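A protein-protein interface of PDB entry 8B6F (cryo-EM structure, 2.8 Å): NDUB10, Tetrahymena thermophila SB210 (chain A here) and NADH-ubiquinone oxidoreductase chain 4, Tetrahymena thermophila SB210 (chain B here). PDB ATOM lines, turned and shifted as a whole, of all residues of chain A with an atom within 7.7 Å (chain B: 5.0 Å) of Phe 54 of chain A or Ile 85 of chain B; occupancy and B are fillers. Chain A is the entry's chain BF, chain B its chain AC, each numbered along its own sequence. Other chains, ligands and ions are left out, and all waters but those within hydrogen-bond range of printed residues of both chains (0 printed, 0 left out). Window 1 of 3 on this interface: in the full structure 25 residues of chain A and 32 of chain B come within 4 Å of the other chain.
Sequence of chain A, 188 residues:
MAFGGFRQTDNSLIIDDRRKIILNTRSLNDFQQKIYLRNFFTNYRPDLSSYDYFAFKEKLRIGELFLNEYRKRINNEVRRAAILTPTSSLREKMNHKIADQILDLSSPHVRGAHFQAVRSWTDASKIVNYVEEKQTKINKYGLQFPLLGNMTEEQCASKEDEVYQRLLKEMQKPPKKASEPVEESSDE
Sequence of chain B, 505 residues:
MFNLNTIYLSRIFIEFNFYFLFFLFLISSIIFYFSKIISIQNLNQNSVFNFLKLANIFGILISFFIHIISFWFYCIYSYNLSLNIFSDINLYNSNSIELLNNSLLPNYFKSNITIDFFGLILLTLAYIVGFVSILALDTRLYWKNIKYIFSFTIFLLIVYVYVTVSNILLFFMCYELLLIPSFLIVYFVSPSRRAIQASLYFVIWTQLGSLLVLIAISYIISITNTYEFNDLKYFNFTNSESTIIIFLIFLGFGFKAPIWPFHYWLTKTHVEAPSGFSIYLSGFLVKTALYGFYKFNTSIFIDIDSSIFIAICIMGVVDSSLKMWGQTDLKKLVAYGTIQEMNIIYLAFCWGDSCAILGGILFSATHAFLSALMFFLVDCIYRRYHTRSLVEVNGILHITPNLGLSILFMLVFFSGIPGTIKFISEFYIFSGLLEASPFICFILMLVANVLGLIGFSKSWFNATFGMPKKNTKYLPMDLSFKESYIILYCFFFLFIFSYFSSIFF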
ATOM      1  N   LEU A  48       9.436 -22.449   9.737  1.00  0.00           N
ATOM      2  CA  LEU A  48       9.957 -23.523   8.908  1.00  0.00           C
ATOM      3  C   LEU A  48      11.434 -23.306   8.600  1.00  0.00           C
ATOM      4  O   LEU A  48      11.933 -22.179   8.603  1.00  0.00           O
ATOM      5  CB  LEU A  48       9.168 -23.612   7.603  1.00  0.00           C
ATOM      6  CG  LEU A  48       7.652 -23.760   7.744  1.00  0.00           C
ATOM      7  CD1 LEU A  48       6.989 -23.771   6.378  1.00  0.00           C
ATOM      8  CD2 LEU A  48       7.299 -25.015   8.519  1.00  0.00           C
ATOM      9  N   SER A  49      12.131 -24.407   8.328  1.00  0.00           N
ATOM     10  CA  SER A  49      13.530 -24.337   7.937  1.00  0.00           C
ATOM     11  C   SER A  49      13.646 -23.789   6.516  1.00  0.00           C
ATOM     12  O   SER A  49      12.656 -23.435   5.871  1.00  0.00           O
ATOM     13  CB  SER A  49      14.180 -25.713   8.046  1.00  0.00           C
ATOM     14  OG  SER A  49      13.566 -26.641   7.169  1.00  0.00           O
ATOM     15  N   SER A  50      14.880 -23.724   6.017  1.00  0.00           N
ATOM     16  CA  SER A  50      15.098 -23.218   4.666  1.00  0.00           C
ATOM     17  C   SER A  50      14.496 -24.163   3.633  1.00  0.00           C
ATOM     18  O   SER A  50      13.797 -23.729   2.712  1.00  0.00           O
ATOM     19  CB  SER A  50      16.591 -23.021   4.413  1.00  0.00           C
ATOM     20  OG  SER A  50      16.819 -22.473   3.127  1.00  0.00           O
ATOM     21  N   TYR A  51      14.764 -25.462   3.770  1.00  0.00           N
ATOM     22  CA  TYR A  51      14.183 -26.435   2.852  1.00  0.00           C
ATOM     23  C   TYR A  51      12.664 -26.448   2.957  1.00  0.00           C
ATOM     24  O   TYR A  51      11.963 -26.464   1.939  1.00  0.00           O
ATOM     25  CB  TYR A  51      14.755 -27.822   3.147  1.00  0.00           C
ATOM     26  CG  TYR A  51      14.254 -28.906   2.224  1.00  0.00           C
ATOM     27  CD1 TYR A  51      13.040 -29.533   2.466  1.00  0.00           C
ATOM     28  CD2 TYR A  51      14.998 -29.321   1.131  1.00  0.00           C
ATOM     29  CE1 TYR A  51      12.573 -30.526   1.642  1.00  0.00           C
ATOM     30  CE2 TYR A  51      14.538 -30.318   0.297  1.00  0.00           C
ATOM     31  CZ  TYR A  51      13.321 -30.913   0.559  1.00  0.00           C
ATOM     32  OH  TYR A  51      12.841 -31.907  -0.252  1.00  0.00           O
ATOM     33  N   ASP A  52      12.139 -26.438   4.183  1.00  0.00           N
ATOM     34  CA  ASP A  52      10.693 -26.471   4.374  1.00  0.00           C
ATOM     35  C   ASP A  52      10.025 -25.234   3.792  1.00  0.00           C
ATOM     36  O   ASP A  52       8.938 -25.325   3.210  1.00  0.00           O
ATOM     37  CB  ASP A  52      10.362 -26.618   5.857  1.00  0.00           C
ATOM     38  CG  ASP A  52      10.671 -28.003   6.386  1.00  0.00           C
ATOM     39  OD1 ASP A  52      10.626 -28.964   5.592  1.00  0.00           O
ATOM     40  OD2 ASP A  52      10.954 -28.133   7.594  1.00  0.00           O
ATOM     41  N   TYR A  53      10.651 -24.067   3.942  1.00  0.00           N
ATOM     42  CA  TYR A  53      10.049 -22.861   3.387  1.00  0.00           C
ATOM     43  C   TYR A  53      10.198 -22.794   1.875  1.00  0.00           C
ATOM     44  O   TYR A  53       9.350 -22.199   1.202  1.00  0.00           O
ATOM     45  CB  TYR A  53      10.647 -21.606   4.015  1.00  0.00           C
ATOM     46  CG  TYR A  53       9.957 -20.362   3.515  1.00  0.00           C
ATOM     47  CD1 TYR A  53       8.770 -19.926   4.090  1.00  0.00           C
ATOM     48  CD2 TYR A  53      10.466 -19.649   2.439  1.00  0.00           C
ATOM     49  CE1 TYR A  53       8.124 -18.801   3.620  1.00  0.00           C
ATOM     50  CE2 TYR A  53       9.827 -18.525   1.965  1.00  0.00           C
ATOM     51  CZ  TYR A  53       8.657 -18.106   2.558  1.00  0.00           C
ATOM     52  OH  TYR A  53       8.019 -16.987   2.087  1.00  0.00           O
ATOM     53  N   PHE A  54      11.254 -23.385   1.314  1.00  0.00           N
ATOM     54  CA  PHE A  54      11.317 -23.491  -0.138  1.00  0.00           C
ATOM     55  C   PHE A  54      10.171 -24.348  -0.656  1.00  0.00           C
ATOM     56  O   PHE A  54       9.531 -24.005  -1.656  1.00  0.00           O
ATOM     57  CB  PHE A  54      12.666 -24.069  -0.569  1.00  0.00           C
ATOM     58  CG  PHE A  54      12.884 -24.052  -2.055  1.00  0.00           C
ATOM     59  CD1 PHE A  54      12.434 -25.093  -2.845  1.00  0.00           C
ATOM     60  CD2 PHE A  54      13.546 -22.999  -2.658  1.00  0.00           C
ATOM     61  CE1 PHE A  54      12.634 -25.083  -4.211  1.00  0.00           C
ATOM     62  CE2 PHE A  54      13.749 -22.981  -4.024  1.00  0.00           C
ATOM     63  CZ  PHE A  54      13.293 -24.026  -4.801  1.00  0.00           C
ATOM     64  N   ALA A  55       9.898 -25.471   0.012  1.00  0.00           N
ATOM     65  CA  ALA A  55       8.749 -26.288  -0.358  1.00  0.00           C
ATOM     66  C   ALA A  55       7.451 -25.508  -0.190  1.00  0.00           C
ATOM     67  O   ALA A  55       6.550 -25.592  -1.032  1.00  0.00           O
ATOM     68  CB  ALA A  55       8.721 -27.564   0.483  1.00  0.00           C
ATOM     69  N   PHE A  56       7.342 -24.742   0.899  1.00  0.00           N
ATOM     70  CA  PHE A  56       6.153 -23.929   1.137  1.00  0.00           C
ATOM     71  C   PHE A  56       5.968 -22.896   0.035  1.00  0.00           C
ATOM     72  O   PHE A  56       4.852 -22.689  -0.452  1.00  0.00           O
ATOM     73  CB  PHE A  56       6.266 -23.247   2.503  1.00  0.00           C
ATOM     74  CG  PHE A  56       5.098 -22.367   2.849  1.00  0.00           C
ATOM     75  CD1 PHE A  56       5.050 -21.050   2.422  1.00  0.00           C
ATOM     76  CD2 PHE A  56       4.065 -22.848   3.634  1.00  0.00           C
ATOM     77  CE1 PHE A  56       3.983 -20.239   2.752  1.00  0.00           C
ATOM     78  CE2 PHE A  56       2.996 -22.041   3.966  1.00  0.00           C
ATOM     79  CZ  PHE A  56       2.957 -20.736   3.525  1.00  0.00           C
ATOM     80  N   LYS A  57       7.055 -22.242  -0.374  1.00  0.00           N
ATOM     81  CA  LYS A  57       6.973 -21.255  -1.443  1.00  0.00           C
ATOM     82  C   LYS A  57       6.533 -21.895  -2.752  1.00  0.00           C
ATOM     83  O   LYS A  57       5.681 -21.352  -3.461  1.00  0.00           O
ATOM     84  CB  LYS A  57       8.329 -20.570  -1.608  1.00  0.00           C
ATOM     85  CG  LYS A  57       8.430 -19.622  -2.793  1.00  0.00           C
ATOM     86  CD  LYS A  57       9.873 -19.229  -3.065  1.00  0.00           C
ATOM     87  CE  LYS A  57      10.674 -20.366  -3.685  1.00  0.00           C
ATOM     88  NZ  LYS A  57      10.134 -20.788  -5.007  1.00  0.00           N
ATOM     89  N   GLU A  58       7.111 -23.046  -3.097  1.00  0.00           N
ATOM     90  CA  GLU A  58       6.715 -23.724  -4.326  1.00  0.00           C
ATOM     91  C   GLU A  58       5.253 -24.144  -4.278  1.00  0.00           C
ATOM     92  O   GLU A  58       4.521 -23.989  -5.262  1.00  0.00           O
ATOM     93  CB  GLU A  58       7.614 -24.935  -4.567  1.00  0.00           C
ATOM     94  CG  GLU A  58       9.056 -24.573  -4.873  1.00  0.00           C
ATOM     95  CD  GLU A  58       9.192 -23.727  -6.123  1.00  0.00           C
ATOM     96  OE1 GLU A  58       8.286 -23.779  -6.980  1.00  0.00           O
ATOM     97  OE2 GLU A  58      10.201 -23.002  -6.245  1.00  0.00           O
ATOM     98  N   LYS A  59       4.802 -24.669  -3.137  1.00  0.00           N
ATOM     99  CA  LYS A  59       3.405 -25.069  -3.013  1.00  0.00           C
ATOM    100  C   LYS A  59       2.480 -23.863  -3.105  1.00  0.00           C
ATOM    101  O   LYS A  59       1.386 -23.956  -3.675  1.00  0.00           O
ATOM    102  CB  LYS A  59       3.192 -25.817  -1.698  1.00  0.00           C
ATOM    103  CG  LYS A  59       3.831 -27.196  -1.672  1.00  0.00           C
ATOM    104  CD  LYS A  59       3.738 -27.826  -0.295  1.00  0.00           C
ATOM    105  CE  LYS A  59       4.429 -29.180  -0.268  1.00  0.00           C
ATOM    106  NZ  LYS A  59       4.460 -29.763   1.104  1.00  0.00           N
ATOM    107  N   LEU A  60       2.893 -22.723  -2.548  1.00  0.00           N
ATOM    108  CA  LEU A  60       2.078 -21.519  -2.658  1.00  0.00           C
ATOM    109  C   LEU A  60       1.979 -21.055  -4.105  1.00  0.00           C
ATOM    110  O   LEU A  60       0.894 -20.689  -4.571  1.00  0.00           O
ATOM    111  CB  LEU A  60       2.657 -20.409  -1.782  1.00  0.00           C
ATOM    112  CG  LEU A  60       1.920 -19.069  -1.812  1.00  0.00           C
ATOM    113  CD1 LEU A  60       0.502 -19.210  -1.280  1.00  0.00           C
ATOM    114  CD2 LEU A  60       2.689 -18.032  -1.017  1.00  0.00           C
ATOM    115  N   GLN A 135      -2.414 -33.037  -3.131  1.00  0.00           N
ATOM    116  CA  GLN A 135      -1.268 -33.919  -3.333  1.00  0.00           C
ATOM    117  C   GLN A 135      -1.454 -35.237  -2.595  1.00  0.00           C
ATOM    118  O   GLN A 135      -1.133 -36.306  -3.126  1.00  0.00           O
ATOM    119  CB  GLN A 135       0.019 -33.238  -2.873  1.00  0.00           C
ATOM    120  CG  GLN A 135       0.554 -32.200  -3.835  1.00  0.00           C
ATOM    121  CD  GLN A 135       1.952 -31.754  -3.465  1.00  0.00           C
ATOM    122  OE1 GLN A 135       2.133 -30.776  -2.743  1.00  0.00           O
ATOM    123  NE2 GLN A 135       2.952 -32.474  -3.958  1.00  0.00           N
ATOM    124  N   ASN A 150       8.942 -37.773  -9.645  1.00  0.00           N
ATOM    125  CA  ASN A 150       9.951 -38.616 -10.267  1.00  0.00           C
ATOM    126  C   ASN A 150      10.265 -39.774  -9.332  1.00  0.00           C
ATOM    127  O   ASN A 150      10.425 -39.578  -8.125  1.00  0.00           O
ATOM    128  CB  ASN A 150      11.233 -37.830 -10.573  1.00  0.00           C
ATOM    129  CG  ASN A 150      11.022 -36.747 -11.608  1.00  0.00           C
ATOM    130  OD1 ASN A 150      10.309 -36.944 -12.590  1.00  0.00           O
ATOM    131  ND2 ASN A 150      11.638 -35.594 -11.391  1.00  0.00           N
ATOM    132  N   LEU B  81      13.593 -30.252 -10.870  1.00  0.00           N
ATOM    133  CA  LEU B  81      13.975 -29.974  -9.488  1.00  0.00           C
ATOM    134  C   LEU B  81      12.793 -29.427  -8.702  1.00  0.00           C
ATOM    135  O   LEU B  81      12.551 -29.845  -7.564  1.00  0.00           O
ATOM    136  CB  LEU B  81      15.153 -28.997  -9.456  1.00  0.00           C
ATOM    137  CG  LEU B  81      15.873 -28.747  -8.122  1.00  0.00           C
ATOM    138  CD1 LEU B  81      17.203 -28.065  -8.375  1.00  0.00           C
ATOM    139  CD2 LEU B  81      15.060 -27.906  -7.143  1.00  0.00           C
ATOM    140  N   SER B  82      12.042 -28.499  -9.292  1.00  0.00           N
ATOM    141  CA  SER B  82      10.834 -28.011  -8.637  1.00  0.00           C
ATOM    142  C   SER B  82       9.840 -29.143  -8.415  1.00  0.00           C
ATOM    143  O   SER B  82       9.211 -29.228  -7.354  1.00  0.00           O
ATOM    144  CB  SER B  82      10.202 -26.899  -9.472  1.00  0.00           C
ATOM    145  OG  SER B  82      11.085 -25.798  -9.604  1.00  0.00           O
ATOM    146  N   LEU B  83       9.684 -30.025  -9.406  1.00  0.00           N
ATOM    147  CA  LEU B  83       8.786 -31.163  -9.243  1.00  0.00           C
ATOM    148  C   LEU B  83       9.250 -32.079  -8.120  1.00  0.00           C
ATOM    149  O   LEU B  83       8.434 -32.562  -7.327  1.00  0.00           O
ATOM    150  CB  LEU B  83       8.677 -31.947 -10.551  1.00  0.00           C
ATOM    151  CG  LEU B  83       7.910 -31.305 -11.709  1.00  0.00           C
ATOM    152  CD1 LEU B  83       7.755 -32.308 -12.838  1.00  0.00           C
ATOM    153  CD2 LEU B  83       6.555 -30.760 -11.284  1.00  0.00           C
ATOM    154  N   ASN B  84      10.557 -32.334  -8.033  1.00  0.00           N
ATOM    155  CA  ASN B  84      11.058 -33.203  -6.974  1.00  0.00           C
ATOM    156  C   ASN B  84      10.788 -32.608  -5.599  1.00  0.00           C
ATOM    157  O   ASN B  84      10.398 -33.325  -4.672  1.00  0.00           O
ATOM    158  CB  ASN B  84      12.556 -33.445  -7.160  1.00  0.00           C
ATOM    159  CG  ASN B  84      12.870 -34.215  -8.424  1.00  0.00           C
ATOM    160  OD1 ASN B  84      12.052 -34.995  -8.910  1.00  0.00           O
ATOM    161  ND2 ASN B  84      14.064 -34.003  -8.963  1.00  0.00           N
ATOM    162  N   ILE B  85      11.004 -31.303  -5.442  1.00  0.00           N
ATOM    163  CA  ILE B  85      10.755 -30.670  -4.153  1.00  0.00           C
ATOM    164  C   ILE B  85       9.266 -30.693  -3.824  1.00  0.00           C
ATOM    165  O   ILE B  85       8.869 -31.001  -2.694  1.00  0.00           O
ATOM    166  CB  ILE B  85      11.311 -29.233  -4.151  1.00  0.00           C
ATOM    167  CG1 ILE B  85      12.832 -29.235  -4.346  1.00  0.00           C
ATOM    168  CG2 ILE B  85      10.934 -28.510  -2.865  1.00  0.00           C
ATOM    169  CD1 ILE B  85      13.619 -29.850  -3.209  1.00  0.00           C
ATOM    170  N   PHE B  86       8.421 -30.372  -4.805  1.00  0.00           N
ATOM    171  CA  PHE B  86       6.998 -30.175  -4.549  1.00  0.00           C
ATOM    172  C   PHE B  86       6.251 -31.493  -4.388  1.00  0.00           C
ATOM    173  O   PHE B  86       5.315 -31.582  -3.586  1.00  0.00           O
ATOM    174  CB  PHE B  86       6.387 -29.350  -5.686  1.00  0.00           C
ATOM    175  CG  PHE B  86       4.892 -29.461  -5.791  1.00  0.00           C
ATOM    176  CD1 PHE B  86       4.072 -28.657  -5.019  1.00  0.00           C
ATOM    177  CD2 PHE B  86       4.308 -30.349  -6.680  1.00  0.00           C
ATOM    178  CE1 PHE B  86       2.698 -28.747  -5.119  1.00  0.00           C
ATOM    179  CE2 PHE B  86       2.932 -30.445  -6.783  1.00  0.00           C
ATOM    180  CZ  PHE B  86       2.126 -29.641  -6.002  1.00  0.00           C
ATOM    181  N   SER B  87       6.645 -32.525  -5.135  1.00  0.00           N
ATOM    182  CA  SER B  87       5.802 -33.712  -5.253  1.00  0.00           C
ATOM    183  C   SER B  87       5.693 -34.457  -3.928  1.00  0.00           C
ATOM    184  O   SER B  87       4.588 -34.776  -3.475  1.00  0.00           O
ATOM    185  CB  SER B  87       6.350 -34.634  -6.342  1.00  0.00           C
ATOM    186  OG  SER B  87       7.663 -35.069  -6.032  1.00  0.00           O
ATOM    187  N   ASP B  88       6.825 -34.747  -3.293  1.00  0.00           N
ATOM    188  CA  ASP B  88       6.822 -35.619  -2.126  1.00  0.00           C
ATOM    189  C   ASP B  88       6.274 -34.888  -0.906  1.00  0.00           C
ATOM    190  O   ASP B  88       6.668 -33.754  -0.619  1.00  0.00           O
ATOM    191  CB  ASP B  88       8.233 -36.129  -1.848  1.00  0.00           C
ATOM    192  CG  ASP B  88       8.244 -37.336  -0.932  1.00  0.00           C
ATOM    193  OD1 ASP B  88       7.161 -37.712  -0.437  1.00  0.00           O
ATOM    194  OD2 ASP B  88       9.329 -37.910  -0.713  1.00  0.00           O
ATOM    195  N   ASN B  95      14.359 -34.378  -0.234  1.00  0.00           N
ATOM    196  CA  ASN B  95      15.212 -34.375  -1.423  1.00  0.00           C
ATOM    197  C   ASN B  95      16.570 -33.798  -1.048  1.00  0.00           C
ATOM    198  O   ASN B  95      16.749 -32.581  -0.990  1.00  0.00           O
ATOM    199  CB  ASN B  95      14.570 -33.580  -2.555  1.00  0.00           C
ATOM    200  CG  ASN B  95      15.463 -33.482  -3.773  1.00  0.00           C
ATOM    201  OD1 ASN B  95      16.405 -34.256  -3.932  1.00  0.00           O
ATOM    202  ND2 ASN B  95      15.170 -32.523  -4.644  1.00  0.00           N
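Ser 49 of chain A touches none of the printed residues of chain B. Of chain B, only Ile 85 comes within 4 Å of Phe 54 of chain A. Of the printed residues of chain A, Asn 84 of chain B touches Asn 150. Of the printed residues of chain A, Asn 95 of chain B touches Tyr 51. The nearest residue of chain B that does not touch Phe 54 of chain A is Leu 81 of chain B (4.7 Å). The nearest printed residue of chain B that does not touch Tyr 51 of chain A is Asn 84 of chain B (5.2 Å).
ND2 of Asn 150 of chain A sits at hydrogen-bond distance from OD1 of Asn 84 of chain B, 2.6 Å away. The side-chain amide nitrogen (NE2) of Gln 135 of chain A is in hydrogen-bond range of the backbone carbonyl oxygen (O) of Phe 86 of chain B (2.6 Å). The backbone carbonyl oxygen of Ser 87 of chain B sits at hydrogen-bond distance from the side-chain amide nitrogen of Gln 135 of chain A (2.9 Å). OH of Tyr 51 of chain A lies within hydrogen-bond range of N of Asn 95 of chain B, at 2.9 Å.
The backbone carbonyl oxygen of Leu 83 of chain B is in hydrogen-bond range of the side-chain hydroxyl of Ser 87 of chain B.
CD1 of Ile 85 of chain B touches CE2 of Tyr 51 of chain A, at 3.7 Å. Phe 54 of chain A touches Ile 85 of chain B. CG2 of Ile 85 of chain B touches CA of Ala 55 of chain A, 3.9996 Å away. Lys 59 of chain A touches Phe 86 of chain B (CG to CD1, 3.7 Å).
Hydrophobic or aromatic side chains of chain A that line the printed part of chain B: Tyr 51 and Phe 54. Hydrophobic or aromatic side chains of chain B within 4 Å of the printed part of chain A: Ile 85 and Phe 86. Among the printed residues, no Asp or Glu carboxylate lies within 4 Å of a Lys or Arg side-chain nitrogen of the other chain.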
